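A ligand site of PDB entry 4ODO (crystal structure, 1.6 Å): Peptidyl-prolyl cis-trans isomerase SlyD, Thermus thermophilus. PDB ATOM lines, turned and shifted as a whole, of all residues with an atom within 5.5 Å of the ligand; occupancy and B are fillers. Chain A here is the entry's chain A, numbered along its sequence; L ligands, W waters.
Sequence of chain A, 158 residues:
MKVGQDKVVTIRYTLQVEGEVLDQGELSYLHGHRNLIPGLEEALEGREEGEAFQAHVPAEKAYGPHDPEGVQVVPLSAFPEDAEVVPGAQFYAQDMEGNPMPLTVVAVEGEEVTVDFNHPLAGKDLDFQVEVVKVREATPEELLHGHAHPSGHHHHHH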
ATOM      1  N   ILE A  11      24.839  36.092  19.725  1.00  0.00           N
ATOM      2  CA  ILE A  11      23.413  36.294  19.517  1.00  0.00           C
ATOM      3  C   ILE A  11      22.609  35.673  20.651  1.00  0.00           C
ATOM      4  O   ILE A  11      23.001  34.655  21.221  1.00  0.00           O
ATOM      5  CB  ILE A  11      22.929  35.698  18.173  1.00  0.00           C
ATOM      6  CG1 ILE A  11      23.259  34.206  18.089  1.00  0.00           C
ATOM      7  CG2 ILE A  11      23.563  36.410  16.986  1.00  0.00           C
ATOM      8  CD1 ILE A  11      22.670  33.513  16.876  1.00  0.00           C
ATOM      9  N   TYR A  13      18.806  34.063  21.019  1.00  0.00           N
ATOM     10  CA  TYR A  13      17.832  33.552  20.073  1.00  0.00           C
ATOM     11  C   TYR A  13      16.730  32.751  20.735  1.00  0.00           C
ATOM     12  O   TYR A  13      16.907  32.195  21.821  1.00  0.00           O
ATOM     13  CB  TYR A  13      18.521  32.672  19.021  1.00  0.00           C
ATOM     14  CG  TYR A  13      19.013  31.362  19.602  1.00  0.00           C
ATOM     15  CD1 TYR A  13      18.219  30.220  19.558  1.00  0.00           C
ATOM     16  CD2 TYR A  13      20.258  31.280  20.210  1.00  0.00           C
ATOM     17  CE1 TYR A  13      18.662  29.031  20.104  1.00  0.00           C
ATOM     18  CE2 TYR A  13      20.713  30.089  20.761  1.00  0.00           C
ATOM     19  CZ  TYR A  13      19.907  28.969  20.703  1.00  0.00           C
ATOM     20  OH  TYR A  13      20.340  27.778  21.234  1.00  0.00           O
ATOM     21  N   LEU A  15      14.063  29.720  19.193  1.00  0.00           N
ATOM     22  CA  LEU A  15      13.659  28.933  18.039  1.00  0.00           C
ATOM     23  C   LEU A  15      12.243  28.430  18.225  1.00  0.00           C
ATOM     24  O   LEU A  15      11.929  27.799  19.227  1.00  0.00           O
ATOM     25  CB  LEU A  15      14.608  27.755  17.821  1.00  0.00           C
ATOM     26  CG  LEU A  15      14.106  26.708  16.823  1.00  0.00           C
ATOM     27  CD1 LEU A  15      13.935  27.314  15.433  1.00  0.00           C
ATOM     28  CD2 LEU A  15      15.028  25.494  16.782  1.00  0.00           C
ATOM     29  N   ASP A  23      13.691  25.911  21.593  1.00  0.00           N
ATOM     30  CA  ASP A  23      14.983  26.227  22.186  1.00  0.00           C
ATOM     31  C   ASP A  23      15.126  27.728  22.352  1.00  0.00           C
ATOM     32  O   ASP A  23      14.444  28.520  21.708  1.00  0.00           O
ATOM     33  CB  ASP A  23      16.124  25.676  21.324  1.00  0.00           C
ATOM     34  CG  ASP A  23      17.474  25.695  22.040  1.00  0.00           C
ATOM     35  OD1 ASP A  23      17.490  25.656  23.283  1.00  0.00           O
ATOM     36  OD2 ASP A  23      18.510  25.740  21.345  1.00  0.00           O
ATOM     37  N   LEU A  27      24.519  32.377  22.058  1.00  0.00           N
ATOM     38  CA  LEU A  27      25.568  31.673  21.332  1.00  0.00           C
ATOM     39  C   LEU A  27      26.580  32.675  20.804  1.00  0.00           C
ATOM     40  O   LEU A  27      26.201  33.750  20.352  1.00  0.00           O
ATOM     41  CB  LEU A  27      24.953  30.865  20.170  1.00  0.00           C
ATOM     42  CG  LEU A  27      25.826  30.481  18.983  1.00  0.00           C
ATOM     43  CD1 LEU A  27      26.664  29.256  19.318  1.00  0.00           C
ATOM     44  CD2 LEU A  27      24.973  30.249  17.744  1.00  0.00           C
ATOM     45  N   ARG A  34      30.629  28.185   7.920  1.00  0.00           N
ATOM     46  CA  ARG A  34      29.635  27.109   7.937  1.00  0.00           C
ATOM     47  C   ARG A  34      29.383  26.571   9.344  1.00  0.00           C
ATOM     48  O   ARG A  34      29.097  25.381   9.533  1.00  0.00           O
ATOM     49  CB  ARG A  34      30.062  25.974   6.971  1.00  0.00           C
ATOM     50  CG  ARG A  34      30.284  26.450   5.534  1.00  0.00           C
ATOM     51  CD  ARG A  34      30.335  25.300   4.511  1.00  0.00           C
ATOM     52  NE  ARG A  34      31.405  24.334   4.793  1.00  0.00           N
ATOM     53  CZ  ARG A  34      31.565  23.188   4.137  1.00  0.00           C
ATOM     54  NH1 ARG A  34      30.748  22.847   3.151  1.00  0.00           N
ATOM     55  NH2 ARG A  34      32.563  22.369   4.469  1.00  0.00           N
ATOM     56  N   ASN A  35      29.444  27.453  10.338  1.00  0.00           N
ATOM     57  CA  ASN A  35      29.169  27.068  11.718  1.00  0.00           C
ATOM     58  C   ASN A  35      27.704  27.235  12.116  1.00  0.00           C
ATOM     59  O   ASN A  35      27.282  26.750  13.179  1.00  0.00           O
ATOM     60  CB  ASN A  35      30.034  27.882  12.680  1.00  0.00           C
ATOM     61  CG  ASN A  35      31.472  27.441  12.686  1.00  0.00           C
ATOM     62  OD1 ASN A  35      31.759  26.245  12.735  1.00  0.00           O
ATOM     63  ND2 ASN A  35      32.379  28.398  12.621  1.00  0.00           N
ATOM     64  N   LEU A  36      26.928  27.902  11.276  1.00  0.00           N
ATOM     65  CA  LEU A  36      25.503  28.098  11.538  1.00  0.00           C
ATOM     66  C   LEU A  36      24.704  27.647  10.319  1.00  0.00           C
ATOM     67  O   LEU A  36      25.254  27.556   9.227  1.00  0.00           O
ATOM     68  CB  LEU A  36      25.208  29.562  11.840  1.00  0.00           C
ATOM     69  CG  LEU A  36      24.804  29.922  13.269  1.00  0.00           C
ATOM     70  CD1 LEU A  36      25.816  29.351  14.255  1.00  0.00           C
ATOM     71  CD2 LEU A  36      24.711  31.423  13.422  1.00  0.00           C
ATOM     72  N   ILE A  37      23.426  27.356  10.509  1.00  0.00           N
ATOM     73  CA  ILE A  37      22.600  27.014   9.361  1.00  0.00           C
ATOM     74  C   ILE A  37      22.651  28.172   8.373  1.00  0.00           C
ATOM     75  O   ILE A  37      22.637  29.346   8.771  1.00  0.00           O
ATOM     76  CB  ILE A  37      21.149  26.670   9.751  1.00  0.00           C
ATOM     77  CG1 ILE A  37      20.558  27.753  10.660  1.00  0.00           C
ATOM     78  CG2 ILE A  37      21.079  25.298  10.435  1.00  0.00           C
ATOM     79  CD1 ILE A  37      19.071  27.557  10.942  1.00  0.00           C
ATOM     80  N   PRO A  38      22.754  27.861   7.069  1.00  0.00           N
ATOM     81  CA  PRO A  38      23.002  28.865   6.033  1.00  0.00           C
ATOM     82  C   PRO A  38      22.010  30.024   6.049  1.00  0.00           C
ATOM     83  O   PRO A  38      22.418  31.178   5.942  1.00  0.00           O
ATOM     84  CB  PRO A  38      22.873  28.055   4.734  1.00  0.00           C
ATOM     85  CG  PRO A  38      23.170  26.667   5.118  1.00  0.00           C
ATOM     86  CD  PRO A  38      22.661  26.501   6.517  1.00  0.00           C
ATOM     87  N   LEU A  40      20.208  31.370   8.431  1.00  0.00           N
ATOM     88  CA  LEU A  40      20.300  32.318   9.544  1.00  0.00           C
ATOM     89  C   LEU A  40      21.539  33.176   9.374  1.00  0.00           C
ATOM     90  O   LEU A  40      21.530  34.376   9.661  1.00  0.00           O
ATOM     91  CB  LEU A  40      20.320  31.600  10.895  1.00  0.00           C
ATOM     92  CG  LEU A  40      20.220  32.563  12.084  1.00  0.00           C
ATOM     93  CD1 LEU A  40      18.971  33.413  11.970  1.00  0.00           C
ATOM     94  CD2 LEU A  40      20.240  31.811  13.403  1.00  0.00           C
ATOM     95  N   ALA A  62      17.852  25.501   6.102  1.00  0.00           N
ATOM     96  CA  ALA A  62      18.037  25.099   7.491  1.00  0.00           C
ATOM     97  C   ALA A  62      18.637  23.704   7.563  1.00  0.00           C
ATOM     98  O   ALA A  62      19.801  23.520   7.204  1.00  0.00           O
ATOM     99  CB  ALA A  62      16.728  25.177   8.255  1.00  0.00           C
ATOM    100  N   TYR A  63      17.862  22.714   7.997  1.00  0.00           N
ATOM    101  CA  TYR A  63      18.399  21.355   8.123  1.00  0.00           C
ATOM    102  C   TYR A  63      18.069  20.455   6.929  1.00  0.00           C
ATOM    103  O   TYR A  63      18.322  19.258   6.966  1.00  0.00           O
ATOM    104  CB  TYR A  63      17.917  20.743   9.436  1.00  0.00           C
ATOM    105  CG  TYR A  63      18.571  21.412  10.613  1.00  0.00           C
ATOM    106  CD1 TYR A  63      17.897  22.367  11.353  1.00  0.00           C
ATOM    107  CD2 TYR A  63      19.892  21.134  10.943  1.00  0.00           C
ATOM    108  CE1 TYR A  63      18.509  23.005  12.415  1.00  0.00           C
ATOM    109  CE2 TYR A  63      20.516  21.769  12.011  1.00  0.00           C
ATOM    110  CZ  TYR A  63      19.811  22.699  12.739  1.00  0.00           C
ATOM    111  OH  TYR A  63      20.423  23.337  13.801  1.00  0.00           O
ATOM    112  N   HIS A 119      17.499  14.198  10.299  1.00  0.00           N
ATOM    113  CA  HIS A 119      17.517  15.198  11.354  1.00  0.00           C
ATOM    114  C   HIS A 119      16.076  15.454  11.790  1.00  0.00           C
ATOM    115  O   HIS A 119      15.182  15.519  10.936  1.00  0.00           O
ATOM    116  CB  HIS A 119      18.179  16.489  10.854  1.00  0.00           C
ATOM    117  CG  HIS A 119      18.475  17.474  11.944  1.00  0.00           C
ATOM    118  ND1 HIS A 119      17.502  18.226  12.551  1.00  0.00           N
ATOM    119  CD2 HIS A 119      19.648  17.831  12.523  1.00  0.00           C
ATOM    120  CE1 HIS A 119      18.053  18.999  13.466  1.00  0.00           C
ATOM    121  NE2 HIS A 119      19.353  18.778  13.467  1.00  0.00           N
ATOM    122  N   LEU A 121      14.590  17.973  12.586  1.00  0.00           N
ATOM    123  CA  LEU A 121      14.052  19.189  11.984  1.00  0.00           C
ATOM    124  C   LEU A 121      14.098  19.187  10.449  1.00  0.00           C
ATOM    125  O   LEU A 121      13.794  20.205   9.818  1.00  0.00           O
ATOM    126  CB  LEU A 121      14.790  20.412  12.522  1.00  0.00           C
ATOM    127  CG  LEU A 121      14.603  20.663  14.016  1.00  0.00           C
ATOM    128  CD1 LEU A 121      15.296  21.954  14.430  1.00  0.00           C
ATOM    129  CD2 LEU A 121      13.109  20.714  14.362  1.00  0.00           C
ATOM    130  N   LEU A 126      12.053  27.036  10.098  1.00  0.00           N
ATOM    131  CA  LEU A 126      12.430  27.485  11.431  1.00  0.00           C
ATOM    132  C   LEU A 126      12.158  28.969  11.596  1.00  0.00           C
ATOM    133  O   LEU A 126      12.472  29.752  10.712  1.00  0.00           O
ATOM    134  CB  LEU A 126      13.905  27.195  11.706  1.00  0.00           C
ATOM    135  CG  LEU A 126      14.402  25.792  11.357  1.00  0.00           C
ATOM    136  CD1 LEU A 126      15.838  25.596  11.818  1.00  0.00           C
ATOM    137  CD2 LEU A 126      13.501  24.719  11.943  1.00  0.00           C
ATOM    138  N   PHE A 128      13.070  32.180  13.931  1.00  0.00           N
ATOM    139  CA  PHE A 128      13.985  32.700  14.944  1.00  0.00           C
ATOM    140  C   PHE A 128      13.666  34.133  15.343  1.00  0.00           C
ATOM    141  O   PHE A 128      13.443  34.976  14.484  1.00  0.00           O
ATOM    142  CB  PHE A 128      15.431  32.651  14.455  1.00  0.00           C
ATOM    143  CG  PHE A 128      16.006  31.263  14.333  1.00  0.00           C
ATOM    144  CD1 PHE A 128      16.581  30.639  15.427  1.00  0.00           C
ATOM    145  CD2 PHE A 128      16.001  30.603  13.116  1.00  0.00           C
ATOM    146  CE1 PHE A 128      17.124  29.375  15.321  1.00  0.00           C
ATOM    147  CE2 PHE A 128      16.540  29.331  13.000  1.00  0.00           C
ATOM    148  CZ  PHE A 128      17.107  28.717  14.099  1.00  0.00           C
HETATM  149  C1  LIG L   1      22.527  26.645  14.457  1.00  0.00           C
HETATM  150  C2  LIG L   1      21.104  27.056  14.789  1.00  0.00           C
HETATM  151  C3  LIG L   1      20.995  28.582  14.662  1.00  0.00           C
HETATM  152  C4  LIG L   1      21.659  29.269  15.858  1.00  0.00           C
HETATM  153  C5  LIG L   1      21.041  28.799  17.166  1.00  0.00           C
HETATM  154  C6  LIG L   1      21.157  27.303  17.271  1.00  0.00           C
HETATM  155  C7  LIG L   1      19.539  25.785  16.173  1.00  0.00           C
HETATM  156  C8  LIG L   1      18.989  25.461  17.545  1.00  0.00           C
HETATM  157  C9  LIG L   1      19.416  24.117  18.174  1.00  0.00           C
HETATM  158  C10 LIG L   1      19.514  22.965  17.167  1.00  0.00           C
HETATM  159  C11 LIG L   1      20.037  21.788  17.931  1.00  0.00           C
HETATM  160  C12 LIG L   1      21.447  22.103  18.393  1.00  0.00           C
HETATM  161  C13 LIG L   1      21.392  23.323  19.363  1.00  0.00           C
HETATM  162  C14 LIG L   1      22.810  23.895  19.639  1.00  0.00           C
HETATM  163  C15 LIG L   1      23.883  22.827  19.944  1.00  0.00           C
HETATM  164  C16 LIG L   1      24.179  22.593  21.436  1.00  0.00           C
HETATM  165  C17 LIG L   1      25.601  22.060  21.624  1.00  0.00           C
HETATM  166  C18 LIG L   1      26.585  22.707  20.701  1.00  0.00           C
HETATM  167  C19 LIG L   1      27.272  21.931  19.879  1.00  0.00           C
HETATM  168  C20 LIG L   1      28.171  22.483  18.841  1.00  0.00           C
HETATM  169  C21 LIG L   1      27.305  22.992  17.705  1.00  0.00           C
HETATM  170  C22 LIG L   1      27.468  24.448  17.406  1.00  0.00           C
HETATM  171  C23 LIG L   1      26.747  24.714  16.082  1.00  0.00           C
HETATM  172  C24 LIG L   1      25.307  25.241  16.301  1.00  0.00           C
HETATM  173  C25 LIG L   1      24.538  25.487  14.991  1.00  0.00           C
HETATM  174  C26 LIG L   1      24.495  24.237  14.148  1.00  0.00           C
HETATM  175  C27 LIG L   1      25.033  24.256  12.948  1.00  0.00           C
HETATM  176  C28 LIG L   1      25.076  23.088  12.009  1.00  0.00           C
HETATM  177  C29 LIG L   1      24.394  23.478  10.703  1.00  0.00           C
HETATM  178  C30 LIG L   1      24.538  22.307   9.709  1.00  0.00           C
HETATM  179  C31 LIG L   1      26.026  22.063   9.478  1.00  0.00           C
HETATM  180  C32 LIG L   1      26.610  21.547  10.780  1.00  0.00           C
HETATM  181  C33 LIG L   1      26.525  22.677  11.801  1.00  0.00           C
HETATM  182  C34 LIG L   1      18.136  22.604  16.667  1.00  0.00           C
HETATM  183  C35 LIG L   1      23.276  21.602  22.134  1.00  0.00           C
HETATM  184  C36 LIG L   1      26.977  24.115  20.994  1.00  0.00           C
HETATM  185  C37 LIG L   1      29.057  21.377  18.273  1.00  0.00           C
HETATM  186  C38 LIG L   1      30.338  21.325  19.064  1.00  0.00           C
HETATM  187  C39 LIG L   1      30.470  20.477  20.064  1.00  0.00           C
HETATM  188  C40 LIG L   1      25.410  26.557  17.068  1.00  0.00           C
HETATM  189  C41 LIG L   1      23.702  23.093  14.688  1.00  0.00           C
HETATM  190  C42 LIG L   1      22.457  20.047  18.250  1.00  0.00           C
HETATM  191  C43 LIG L   1      23.273  26.012  20.409  1.00  0.00           C
HETATM  192  C44 LIG L   1      22.650  22.429   8.414  1.00  0.00           C
HETATM  193  N1  LIG L   1      20.565  26.651  16.085  1.00  0.00           N
HETATM  194  O1  LIG L   1      23.213  25.908  15.353  1.00  0.00           O
HETATM  195  O2  LIG L   1      23.032  26.927  13.373  1.00  0.00           O
HETATM  196  O3  LIG L   1      19.057  25.293  15.140  1.00  0.00           O
HETATM  197  O4  LIG L   1      18.262  26.222  18.108  1.00  0.00           O
HETATM  198  O5  LIG L   1      20.657  24.397  18.797  1.00  0.00           O
HETATM  199  O6  LIG L   1      18.527  23.793  19.210  1.00  0.00           O
HETATM  200  O7  LIG L   1      21.849  20.954  19.124  1.00  0.00           O
HETATM  201  O8  LIG L   1      22.710  24.754  20.746  1.00  0.00           O
HETATM  202  O9  LIG L   1      26.550  22.294  17.120  1.00  0.00           O
HETATM  203  O10 LIG L   1      27.506  25.655  15.354  1.00  0.00           O
HETATM  204  O11 LIG L   1      24.011  22.761   8.487  1.00  0.00           O
HETATM  205  O12 LIG L   1      26.084  21.086   8.475  1.00  0.00           O
HETATM  206  O   HOH W   1      21.024  24.486  22.689  1.00  0.00           O
HETATM  207  O   HOH W   2      29.772  23.957  13.913  1.00  0.00           O
HETATM  208  O   HOH W   3      28.427  22.435   6.268  1.00  0.00           O
HETATM  209  O   HOH W   4      25.690  19.816  16.159  1.00  0.00           O
HETATM  210  O   HOH W   5      20.414  19.889  21.220  1.00  0.00           O
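Water W1 lies within hydrogen-bond range of O8 of the ligand (2.6 Å) and OD2 of Asp 23 (3.1 Å). Water W2 bridges an oxygen (O10) of the ligand and the side-chain amide oxygen (OD1) of Asn 35.
The side-chain carboxylate (OD2) of Asp 23 sits at hydrogen-bond distance from an oxygen (O6) of the ligand (2.9 Å). The backbone NH of Ile 37 sits at hydrogen-bond distance from an oxygen (O2) of the ligand, at 2.9 Å. An oxygen (O10) of the ligand sits at hydrogen-bond distance from the backbone carbonyl oxygen (O) of Asn 35, at 2.4 Å. An oxygen (O3) of the ligand lies within hydrogen-bond range of the side-chain hydroxyl of Tyr 63, 2.7 Å away.
The side-chain carboxylate (OD2) of Asp 23 sits at hydrogen-bond distance from the side-chain hydroxyl (OH) of Tyr 13 (2.7 Å). O of Asp 23 lies within hydrogen-bond range of N of Leu 15 (2.8 Å). The backbone carbonyl oxygen of Leu 27 is in hydrogen-bond range of the backbone NH of Ile 11, at 2.8 Å. The backbone NH (N) of Leu 121 lies within hydrogen-bond range of a ring nitrogen (ND1) of His 119 (2.9 Å).
Tyr 13 touches the ligand (CE1 to O4, 3.5 Å). Leu 15 touches the ligand (CD2 to O4, 3.6 Å). Leu 27 touches the ligand. CA of Leu 36 touches O2 of the ligand, 3.3 Å away. Leu 40 touches the ligand. Ala 62 touches the ligand. Leu 121 touches the ligand (CD1 to C34, 3.7 Å). Phe 128 touches the ligand. Hydrophobic or aromatic side chains that line the ligand: Tyr 13, Leu 15, Leu 27, Leu 36, Ile 37, Leu 40, Tyr 63, Leu 121 and Phe 128. Of the 17 residues printed, 12 come within 4 Å of the ligand.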
